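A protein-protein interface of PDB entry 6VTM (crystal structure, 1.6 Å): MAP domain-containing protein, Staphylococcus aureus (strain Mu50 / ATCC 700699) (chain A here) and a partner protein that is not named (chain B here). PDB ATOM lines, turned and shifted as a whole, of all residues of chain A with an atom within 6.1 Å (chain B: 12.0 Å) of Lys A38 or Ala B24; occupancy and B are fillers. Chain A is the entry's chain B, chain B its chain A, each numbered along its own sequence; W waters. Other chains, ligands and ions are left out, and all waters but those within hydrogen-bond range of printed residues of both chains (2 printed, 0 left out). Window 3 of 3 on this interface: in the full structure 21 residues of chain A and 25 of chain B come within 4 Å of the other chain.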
ATOM      1  N   TYR A  21     -10.599  -9.223  -9.512  1.00  0.00           N
ATOM      2  CA  TYR A  21      -9.265  -9.661  -9.912  1.00  0.00           C
ATOM      3  C   TYR A  21      -8.810  -8.957 -11.187  1.00  0.00           C
ATOM      4  O   TYR A  21      -9.596  -8.737 -12.114  1.00  0.00           O
ATOM      5  CB  TYR A  21      -9.215 -11.202 -10.203  1.00  0.00           C
ATOM      6  CG  TYR A  21      -9.935 -12.117  -9.270  1.00  0.00           C
ATOM      7  CD1 TYR A  21     -11.300 -12.300  -9.375  1.00  0.00           C
ATOM      8  CD2 TYR A  21      -9.245 -12.850  -8.316  1.00  0.00           C
ATOM      9  CE1 TYR A  21     -11.972 -13.139  -8.516  1.00  0.00           C
ATOM     10  CE2 TYR A  21      -9.907 -13.689  -7.442  1.00  0.00           C
ATOM     11  CZ  TYR A  21     -11.271 -13.838  -7.558  1.00  0.00           C
ATOM     12  OH  TYR A  21     -11.952 -14.682  -6.719  1.00  0.00           O
ATOM     13  N   PHE A  22      -7.502  -8.705 -11.279  1.00  0.00           N
ATOM     14  CA  PHE A  22      -6.914  -8.397 -12.579  1.00  0.00           C
ATOM     15  C   PHE A  22      -6.423  -9.700 -13.225  1.00  0.00           C
ATOM     16  O   PHE A  22      -5.979 -10.618 -12.535  1.00  0.00           O
ATOM     17  CB  PHE A  22      -5.723  -7.445 -12.468  1.00  0.00           C
ATOM     18  CG  PHE A  22      -6.034  -6.065 -12.038  1.00  0.00           C
ATOM     19  CD1 PHE A  22      -6.901  -5.293 -12.760  1.00  0.00           C
ATOM     20  CD2 PHE A  22      -5.401  -5.516 -10.951  1.00  0.00           C
ATOM     21  CE1 PHE A  22      -7.149  -3.986 -12.400  1.00  0.00           C
ATOM     22  CE2 PHE A  22      -5.655  -4.222 -10.561  1.00  0.00           C
ATOM     23  CZ  PHE A  22      -6.527  -3.451 -11.298  1.00  0.00           C
ATOM     24  N   VAL A  23      -6.462  -9.750 -14.551  1.00  0.00           N
ATOM     25  CA  VAL A  23      -5.855 -10.852 -15.306  1.00  0.00           C
ATOM     26  C   VAL A  23      -4.739 -10.297 -16.180  1.00  0.00           C
ATOM     27  O   VAL A  23      -4.975  -9.408 -17.008  1.00  0.00           O
ATOM     28  CB  VAL A  23      -6.910 -11.589 -16.142  1.00  0.00           C
ATOM     29  CG1 VAL A  23      -6.249 -12.682 -16.961  1.00  0.00           C
ATOM     30  CG2 VAL A  23      -7.985 -12.146 -15.202  1.00  0.00           C
ATOM     31  N   PHE A  24      -3.540 -10.809 -15.987  1.00  0.00           N
ATOM     32  CA  PHE A  24      -2.363 -10.498 -16.785  1.00  0.00           C
ATOM     33  C   PHE A  24      -1.994 -11.689 -17.660  1.00  0.00           C
ATOM     34  O   PHE A  24      -2.066 -12.830 -17.198  1.00  0.00           O
ATOM     35  CB  PHE A  24      -1.160 -10.164 -15.888  1.00  0.00           C
ATOM     36  CG  PHE A  24      -1.371  -8.958 -15.025  1.00  0.00           C
ATOM     37  CD1 PHE A  24      -1.086  -7.700 -15.485  1.00  0.00           C
ATOM     38  CD2 PHE A  24      -1.846  -9.106 -13.750  1.00  0.00           C
ATOM     39  CE1 PHE A  24      -1.290  -6.596 -14.676  1.00  0.00           C
ATOM     40  CE2 PHE A  24      -2.068  -8.009 -12.932  1.00  0.00           C
ATOM     41  CZ  PHE A  24      -1.803  -6.754 -13.391  1.00  0.00           C
ATOM     42  N   GLN A  33       4.010   2.030 -14.457  1.00  0.00           N
ATOM     43  CA  GLN A  33       3.036   3.003 -14.936  1.00  0.00           C
ATOM     44  C   GLN A  33       1.823   2.311 -15.548  1.00  0.00           C
ATOM     45  O   GLN A  33       0.713   2.855 -15.492  1.00  0.00           O
ATOM     46  CB  GLN A  33       3.678   3.969 -15.931  1.00  0.00           C
ATOM     47  CG  GLN A  33       4.091   3.317 -17.214  1.00  0.00           C
ATOM     48  CD  GLN A  33       4.648   4.325 -18.228  1.00  0.00           C
ATOM     49  OE1 GLN A  33       4.977   5.461 -17.882  1.00  0.00           O
ATOM     50  NE2 GLN A  33       4.731   3.909 -19.483  1.00  0.00           N
ATOM     51  N   GLU A  34       1.993   1.105 -16.112  1.00  0.00           N
ATOM     52  CA  GLU A  34       0.831   0.393 -16.639  1.00  0.00           C
ATOM     53  C   GLU A  34      -0.072  -0.102 -15.510  1.00  0.00           C
ATOM     54  O   GLU A  34      -1.298  -0.112 -15.656  1.00  0.00           O
ATOM     55  CB  GLU A  34       1.263  -0.770 -17.515  1.00  0.00           C
ATOM     56  CG  GLU A  34       1.940  -0.347 -18.784  1.00  0.00           C
ATOM     57  CD  GLU A  34       2.472  -1.533 -19.545  1.00  0.00           C
ATOM     58  OE1 GLU A  34       1.650  -2.292 -20.096  1.00  0.00           O
ATOM     59  OE2 GLU A  34       3.723  -1.705 -19.571  1.00  0.00           O
ATOM     60  N   ILE A  35       0.520  -0.560 -14.401  1.00  0.00           N
ATOM     61  CA  ILE A  35      -0.267  -0.911 -13.218  1.00  0.00           C
ATOM     62  C   ILE A  35      -0.910   0.326 -12.621  1.00  0.00           C
ATOM     63  O   ILE A  35      -2.067   0.280 -12.190  1.00  0.00           O
ATOM     64  CB  ILE A  35       0.601  -1.638 -12.182  1.00  0.00           C
ATOM     65  CG1 ILE A  35       1.313  -2.851 -12.820  1.00  0.00           C
ATOM     66  CG2 ILE A  35      -0.238  -2.038 -10.974  1.00  0.00           C
ATOM     67  CD1 ILE A  35       2.060  -3.697 -11.855  1.00  0.00           C
ATOM     68  N   ASP A  36      -0.189   1.449 -12.585  1.00  0.00           N
ATOM     69  CA  ASP A  36      -0.797   2.702 -12.123  1.00  0.00           C
ATOM     70  C   ASP A  36      -2.063   3.003 -12.932  1.00  0.00           C
ATOM     71  O   ASP A  36      -3.089   3.421 -12.380  1.00  0.00           O
ATOM     72  CB  ASP A  36       0.198   3.881 -12.258  1.00  0.00           C
ATOM     73  CG  ASP A  36       1.473   3.705 -11.443  1.00  0.00           C
ATOM     74  OD1 ASP A  36       1.480   2.867 -10.535  1.00  0.00           O
ATOM     75  OD2 ASP A  36       2.464   4.449 -11.700  1.00  0.00           O
ATOM     76  N   SER A  37      -1.984   2.839 -14.269  1.00  0.00           N
ATOM     77  CA  SER A  37      -3.125   3.115 -15.142  1.00  0.00           C
ATOM     78  C   SER A  37      -4.271   2.164 -14.853  1.00  0.00           C
ATOM     79  O   SER A  37      -5.418   2.603 -14.753  1.00  0.00           O
ATOM     80  CB  SER A  37      -2.744   3.017 -16.626  1.00  0.00           C
ATOM     81  OG  SER A  37      -1.680   3.915 -16.933  1.00  0.00           O
ATOM     82  N   LYS A  38      -3.986   0.869 -14.698  1.00  0.00           N
ATOM     83  CA  LYS A  38      -5.053  -0.081 -14.395  1.00  0.00           C
ATOM     84  C   LYS A  38      -5.730   0.294 -13.087  1.00  0.00           C
ATOM     85  O   LYS A  38      -6.962   0.305 -13.000  1.00  0.00           O
ATOM     86  CB  LYS A  38      -4.534  -1.521 -14.331  1.00  0.00           C
ATOM     87  CG  LYS A  38      -4.164  -2.161 -15.675  1.00  0.00           C
ATOM     88  CD  LYS A  38      -3.962  -3.695 -15.475  1.00  0.00           C
ATOM     89  CE  LYS A  38      -3.524  -4.442 -16.748  1.00  0.00           C
ATOM     90  NZ  LYS A  38      -4.522  -4.326 -17.820  1.00  0.00           N
ATOM     91  N   VAL A  39      -4.937   0.656 -12.084  1.00  0.00           N
ATOM     92  CA  VAL A  39      -5.492   1.027 -10.784  1.00  0.00           C
ATOM     93  C   VAL A  39      -6.368   2.269 -10.893  1.00  0.00           C
ATOM     94  O   VAL A  39      -7.502   2.292 -10.389  1.00  0.00           O
ATOM     95  CB  VAL A  39      -4.353   1.219  -9.765  1.00  0.00           C
ATOM     96  CG1 VAL A  39      -4.902   1.932  -8.502  1.00  0.00           C
ATOM     97  CG2 VAL A  39      -3.793  -0.129  -9.416  1.00  0.00           C
ATOM     98  N   LYS A  40      -5.862   3.339 -11.515  1.00  0.00           N
ATOM     99  CA  LYS A  40      -6.664   4.551 -11.655  1.00  0.00           C
ATOM    100  C   LYS A  40      -7.900   4.312 -12.508  1.00  0.00           C
ATOM    101  O   LYS A  40      -8.965   4.882 -12.231  1.00  0.00           O
ATOM    102  CB  LYS A  40      -5.845   5.688 -12.254  1.00  0.00           C
ATOM    103  CG  LYS A  40      -4.746   6.121 -11.343  1.00  0.00           C
ATOM    104  CD  LYS A  40      -4.114   7.435 -11.787  1.00  0.00           C
ATOM    105  CE  LYS A  40      -3.263   7.255 -12.997  1.00  0.00           C
ATOM    106  NZ  LYS A  40      -2.149   8.254 -12.973  1.00  0.00           N
ATOM    107  N   ASN A  41      -7.797   3.436 -13.513  1.00  0.00           N
ATOM    108  CA  ASN A  41      -8.969   3.122 -14.332  1.00  0.00           C
ATOM    109  C   ASN A  41     -10.056   2.446 -13.508  1.00  0.00           C
ATOM    110  O   ASN A  41     -11.247   2.736 -13.704  1.00  0.00           O
ATOM    111  CB  ASN A  41      -8.576   2.230 -15.517  1.00  0.00           C
ATOM    112  CG  ASN A  41      -7.777   2.961 -16.556  1.00  0.00           C
ATOM    113  OD1 ASN A  41      -7.657   4.196 -16.533  1.00  0.00           O
ATOM    114  ND2 ASN A  41      -7.177   2.190 -17.461  1.00  0.00           N
ATOM    115  N   GLU A  42      -9.677   1.547 -12.593  1.00  0.00           N
ATOM    116  CA  GLU A  42     -10.666   0.891 -11.735  1.00  0.00           C
ATOM    117  C   GLU A  42     -11.196   1.848 -10.670  1.00  0.00           C
ATOM    118  O   GLU A  42     -12.392   1.828 -10.350  1.00  0.00           O
ATOM    119  CB  GLU A  42     -10.101  -0.360 -11.064  1.00  0.00           C
ATOM    120  CG  GLU A  42      -9.787  -1.499 -12.043  1.00  0.00           C
ATOM    121  CD  GLU A  42     -10.960  -1.885 -12.948  1.00  0.00           C
ATOM    122  OE1 GLU A  42     -12.099  -1.926 -12.461  1.00  0.00           O
ATOM    123  OE2 GLU A  42     -10.763  -2.204 -14.145  1.00  0.00           O
ATOM    124  N   LEU A  43     -10.341   2.714 -10.135  1.00  0.00           N
ATOM    125  CA  LEU A  43     -10.832   3.757  -9.234  1.00  0.00           C
ATOM    126  C   LEU A  43     -11.913   4.593  -9.915  1.00  0.00           C
ATOM    127  O   LEU A  43     -12.936   4.912  -9.296  1.00  0.00           O
ATOM    128  CB  LEU A  43      -9.683   4.635  -8.753  1.00  0.00           C
ATOM    129  CG  LEU A  43      -8.822   3.954  -7.697  1.00  0.00           C
ATOM    130  CD1 LEU A  43      -7.593   4.760  -7.492  1.00  0.00           C
ATOM    131  CD2 LEU A  43      -9.530   3.846  -6.347  1.00  0.00           C
ATOM    132  N   ILE B  20     -18.581 -12.125 -13.541  1.00  0.00           N
ATOM    133  CA  ILE B  20     -18.756 -10.848 -14.220  1.00  0.00           C
ATOM    134  C   ILE B  20     -17.485 -10.497 -14.980  1.00  0.00           C
ATOM    135  O   ILE B  20     -16.394 -10.540 -14.413  1.00  0.00           O
ATOM    136  CB  ILE B  20     -19.088  -9.726 -13.224  1.00  0.00           C
ATOM    137  CG1 ILE B  20     -20.382 -10.023 -12.451  1.00  0.00           C
ATOM    138  CG2 ILE B  20     -19.213  -8.435 -13.938  1.00  0.00           C
ATOM    139  CD1 ILE B  20     -20.172 -10.051 -10.980  1.00  0.00           C
ATOM    140  N   GLN B  21     -17.623 -10.125 -16.247  1.00  0.00           N
ATOM    141  CA  GLN B  21     -16.463  -9.680 -17.032  1.00  0.00           C
ATOM    142  C   GLN B  21     -16.242  -8.184 -16.882  1.00  0.00           C
ATOM    143  O   GLN B  21     -17.178  -7.395 -17.024  1.00  0.00           O
ATOM    144  CB  GLN B  21     -16.665 -10.006 -18.507  1.00  0.00           C
ATOM    145  CG  GLN B  21     -15.469  -9.682 -19.365  1.00  0.00           C
ATOM    146  CD  GLN B  21     -14.317 -10.571 -19.037  1.00  0.00           C
ATOM    147  OE1 GLN B  21     -14.423 -11.804 -19.110  1.00  0.00           O
ATOM    148  NE2 GLN B  21     -13.199  -9.965 -18.641  1.00  0.00           N
ATOM    149  N   SER B  22     -14.999  -7.793 -16.647  1.00  0.00           N
ATOM    150  CA  SER B  22     -14.605  -6.395 -16.610  1.00  0.00           C
ATOM    151  C   SER B  22     -13.485  -6.109 -17.613  1.00  0.00           C
ATOM    152  O   SER B  22     -12.948  -7.041 -18.212  1.00  0.00           O
ATOM    153  CB  SER B  22     -14.167  -6.024 -15.202  1.00  0.00           C
ATOM    154  OG  SER B  22     -15.204  -6.306 -14.281  1.00  0.00           O
ATOM    155  N   PRO B  23     -13.111  -4.842 -17.814  1.00  0.00           N
ATOM    156  CA  PRO B  23     -12.160  -4.527 -18.899  1.00  0.00           C
ATOM    157  C   PRO B  23     -10.769  -5.105 -18.705  1.00  0.00           C
ATOM    158  O   PRO B  23     -10.069  -5.358 -19.700  1.00  0.00           O
ATOM    159  CB  PRO B  23     -12.116  -2.992 -18.898  1.00  0.00           C
ATOM    160  CG  PRO B  23     -13.286  -2.557 -18.049  1.00  0.00           C
ATOM    161  CD  PRO B  23     -13.557  -3.639 -17.101  1.00  0.00           C
ATOM    162  N   ALA B  24     -10.338  -5.327 -17.457  1.00  0.00           N
ATOM    163  CA  ALA B  24      -8.977  -5.743 -17.138  1.00  0.00           C
ATOM    164  C   ALA B  24      -8.969  -6.960 -16.210  1.00  0.00           C
ATOM    165  O   ALA B  24      -7.929  -7.303 -15.625  1.00  0.00           O
ATOM    166  CB  ALA B  24      -8.204  -4.568 -16.524  1.00  0.00           C
ATOM    167  N   GLY B  25     -10.092  -7.663 -16.113  1.00  0.00           N
ATOM    168  CA  GLY B  25     -10.157  -8.852 -15.286  1.00  0.00           C
ATOM    169  C   GLY B  25     -11.600  -9.251 -15.105  1.00  0.00           C
ATOM    170  O   GLY B  25     -12.420  -9.068 -16.004  1.00  0.00           O
ATOM    171  N   GLN B  26     -11.906  -9.759 -13.928  1.00  0.00           N
ATOM    172  CA  GLN B  26     -13.246 -10.264 -13.686  1.00  0.00           C
ATOM    173  C   GLN B  26     -13.635  -9.997 -12.249  1.00  0.00           C
ATOM    174  O   GLN B  26     -12.792  -9.684 -11.408  1.00  0.00           O
ATOM    175  CB  GLN B  26     -13.347 -11.751 -13.969  1.00  0.00           C
ATOM    176  CG  GLN B  26     -13.295 -12.034 -15.438  1.00  0.00           C
ATOM    177  CD  GLN B  26     -13.680 -13.447 -15.762  1.00  0.00           C
ATOM    178  OE1 GLN B  26     -13.839 -14.271 -14.868  1.00  0.00           O
ATOM    179  NE2 GLN B  26     -13.888 -13.729 -17.050  1.00  0.00           N
ATOM    180  N   SER B  27     -14.927 -10.135 -11.967  1.00  0.00           N
ATOM    181  CA  SER B  27     -15.388 -10.028 -10.596  1.00  0.00           C
ATOM    182  C   SER B  27     -16.324 -11.183 -10.286  1.00  0.00           C
ATOM    183  O   SER B  27     -16.801 -11.887 -11.176  1.00  0.00           O
ATOM    184  CB  SER B  27     -16.065  -8.682 -10.288  1.00  0.00           C
ATOM    185  OG  SER B  27     -17.103  -8.366 -11.162  1.00  0.00           O
ATOM    186  N   ARG B  28     -16.493 -11.325  -8.919  1.00  0.00           N
ATOM    187  CA  ARG B  28     -17.396 -12.369  -8.467  1.00  0.00           C
ATOM    188  C   ARG B  28     -18.356 -11.788  -7.454  1.00  0.00           C
ATOM    189  O   ARG B  28     -17.987 -10.952  -6.623  1.00  0.00           O
ATOM    190  CB  ARG B  28     -16.696 -13.547  -7.860  1.00  0.00           C
ATOM    191  CG  ARG B  28     -15.757 -14.277  -8.688  1.00  0.00           C
ATOM    192  CD  ARG B  28     -16.531 -15.079  -9.745  1.00  0.00           C
ATOM    193  NE  ARG B  28     -15.673 -15.892 -10.608  1.00  0.00           N
ATOM    194  CZ  ARG B  28     -15.174 -15.478 -11.774  1.00  0.00           C
ATOM    195  NH1 ARG B  28     -15.447 -14.257 -12.240  1.00  0.00           N
ATOM    196  NH2 ARG B  28     -14.409 -16.290 -12.488  1.00  0.00           N
ATOM    197  N   TRP B  46     -22.085  -4.802 -11.738  1.00  0.00           N
ATOM    198  CA  TRP B  46     -22.334  -4.728 -13.166  1.00  0.00           C
ATOM    199  C   TRP B  46     -21.077  -5.015 -13.962  1.00  0.00           C
ATOM    200  O   TRP B  46     -19.957  -4.625 -13.588  1.00  0.00           O
ATOM    201  CB  TRP B  46     -22.836  -3.345 -13.480  1.00  0.00           C
ATOM    202  CG  TRP B  46     -23.428  -3.071 -14.768  1.00  0.00           C
ATOM    203  CD1 TRP B  46     -24.537  -3.658 -15.326  1.00  0.00           C
ATOM    204  CD2 TRP B  46     -23.064  -1.998 -15.623  1.00  0.00           C
ATOM    205  NE1 TRP B  46     -24.844  -3.042 -16.511  1.00  0.00           N
ATOM    206  CE2 TRP B  46     -23.958  -2.010 -16.711  1.00  0.00           C
ATOM    207  CE3 TRP B  46     -22.049  -1.033 -15.586  1.00  0.00           C
ATOM    208  CZ2 TRP B  46     -23.862  -1.098 -17.755  1.00  0.00           C
ATOM    209  CZ3 TRP B  46     -21.952  -0.131 -16.625  1.00  0.00           C
ATOM    210  CH2 TRP B  46     -22.856  -0.165 -17.692  1.00  0.00           C
ATOM    211  N   GLY B  47     -21.276  -5.672 -15.099  1.00  0.00           N
ATOM    212  CA  GLY B  47     -20.186  -5.852 -16.028  1.00  0.00           C
ATOM    213  C   GLY B  47     -20.718  -6.244 -17.386  1.00  0.00           C
ATOM    214  O   GLY B  47     -21.928  -6.420 -17.576  1.00  0.00           O
ATOM    215  N   SER B  48     -19.746  -6.503 -18.268  1.00  0.00           N
ATOM    216  CA  SER B  48     -19.817  -6.570 -19.731  1.00  0.00           C
ATOM    217  C   SER B  48     -19.887  -8.001 -20.206  1.00  0.00           C
ATOM    218  O   SER B  48     -19.138  -8.397 -21.100  1.00  0.00           O
ATOM    219  CB  SER B  48     -18.587  -5.922 -20.365  1.00  0.00           C
ATOM    220  OG  SER B  48     -18.697  -6.064 -21.779  1.00  0.00           O
ATOM    221  N   ASN B  49     -20.709  -8.783 -19.522  1.00  0.00           N
ATOM    222  CA  ASN B  49     -21.071 -10.185 -19.702  1.00  0.00           C
ATOM    223  C   ASN B  49     -21.273 -10.649 -18.250  1.00  0.00           C
ATOM    224  O   ASN B  49     -20.311 -10.543 -17.459  1.00  0.00           O
ATOM    225  CB  ASN B  49     -20.007 -11.096 -20.346  1.00  0.00           C
ATOM    226  CG  ASN B  49     -19.872 -10.924 -21.852  1.00  0.00           C
ATOM    227  OD1 ASN B  49     -20.856 -10.754 -22.583  1.00  0.00           O
ATOM    228  ND2 ASN B  49     -18.641 -11.010 -22.329  1.00  0.00           N
HETATM  229  O   HOH W   1     -11.178  -4.721 -14.788  1.00  0.00           O
HETATM  230  O   HOH W   2      -5.209  -6.864 -16.072  1.00  0.00           O
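OE1 of Gln B26 lies within hydrogen-bond range of NH1 of Arg B28 (3.1 Å). OE1 of Gln B21 is in hydrogen-bond range of NE2 of Gln B26 (2.9 Å). The side-chain amide nitrogen of Gln B21 sits at hydrogen-bond distance from the backbone carbonyl oxygen of Gly B25 (2.9 Å).
O of Tyr A21 touches CA of Gly B25 (3.2 Å). Tyr A21 touches Arg B28. Phe A22 touches Ala B24. N of Val A23 touches CA of Gly B25, at 3.9 Å. Ala B24 touches Lys A38 (CB to NZ, 3.9 Å).
Of the printed residues of chain B, Tyr A21 touches Gly B25, Gln B26 and Arg B28. Of chain B, only Ala B24 comes within 4 Å of Phe A22. Val A23 touches just these residues of chain B: Ala B24 and Gly B25. No residue of chain B comes within 4 Å of Ser A37. Printed residues of chain B within 4 Å of Lys A38: Ala B24 (3.9 Å). No residue of chain B comes within 4 Å of Val A39. No residue of chain B comes within 4 Å of Lys A40. Of chain A, only Phe A22 (3.4 Å), Val A23 (3.0 Å) and Lys A38 (3.9 Å) come within 4 Å of Ala B24. Of the printed residues of chain A, Gly B25 touches Tyr A21 and Val A23. Printed residues of chain A within 4 Å of Gln B26: Tyr A21 (2.9 Å). Printed residues of chain A within 4 Å of Arg B28: Tyr A21. Ser B48 touches none of the printed residues of chain A.
Of the 13 printed residues of chain B, 4 touch a printed residue of chain A. Hydrophobic or aromatic side chains of chain B that line the printed part of chain A: Ala B24. Of the 15 printed residues of chain A, 4 touch a printed residue of chain B. Hydrophobic or aromatic side chains of chain A that line the printed part of chain B: Tyr A21, Phe A22 and Val A23. Among the printed residues, no Asp or Glu carboxylate lies within 4 Å of a Lys or Arg side-chain nitrogen of the other chain.
O of Ala B24 sits at hydrogen-bond distance from N of Val A23, at 3.0 Å. The backbone NH (N) of Tyr A21 is in hydrogen-bond range of the backbone carbonyl oxygen (O) of Gln B26.
Water W1 lies within hydrogen-bond range of the side-chain carboxylate (OE2) of Glu A42 (2.6 Å), the backbone NH (N) of Ala B24 (2.9 Å) and the backbone NH (N) of Gly B25 (3.4 Å). Water W2 lies within hydrogen-bond range of the backbone carbonyl oxygen of Val A23 (2.7 Å), the backbone carbonyl oxygen of Ala B24 (2.8 Å) and the side-chain amino group of Lys A38 (3.2 Å).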
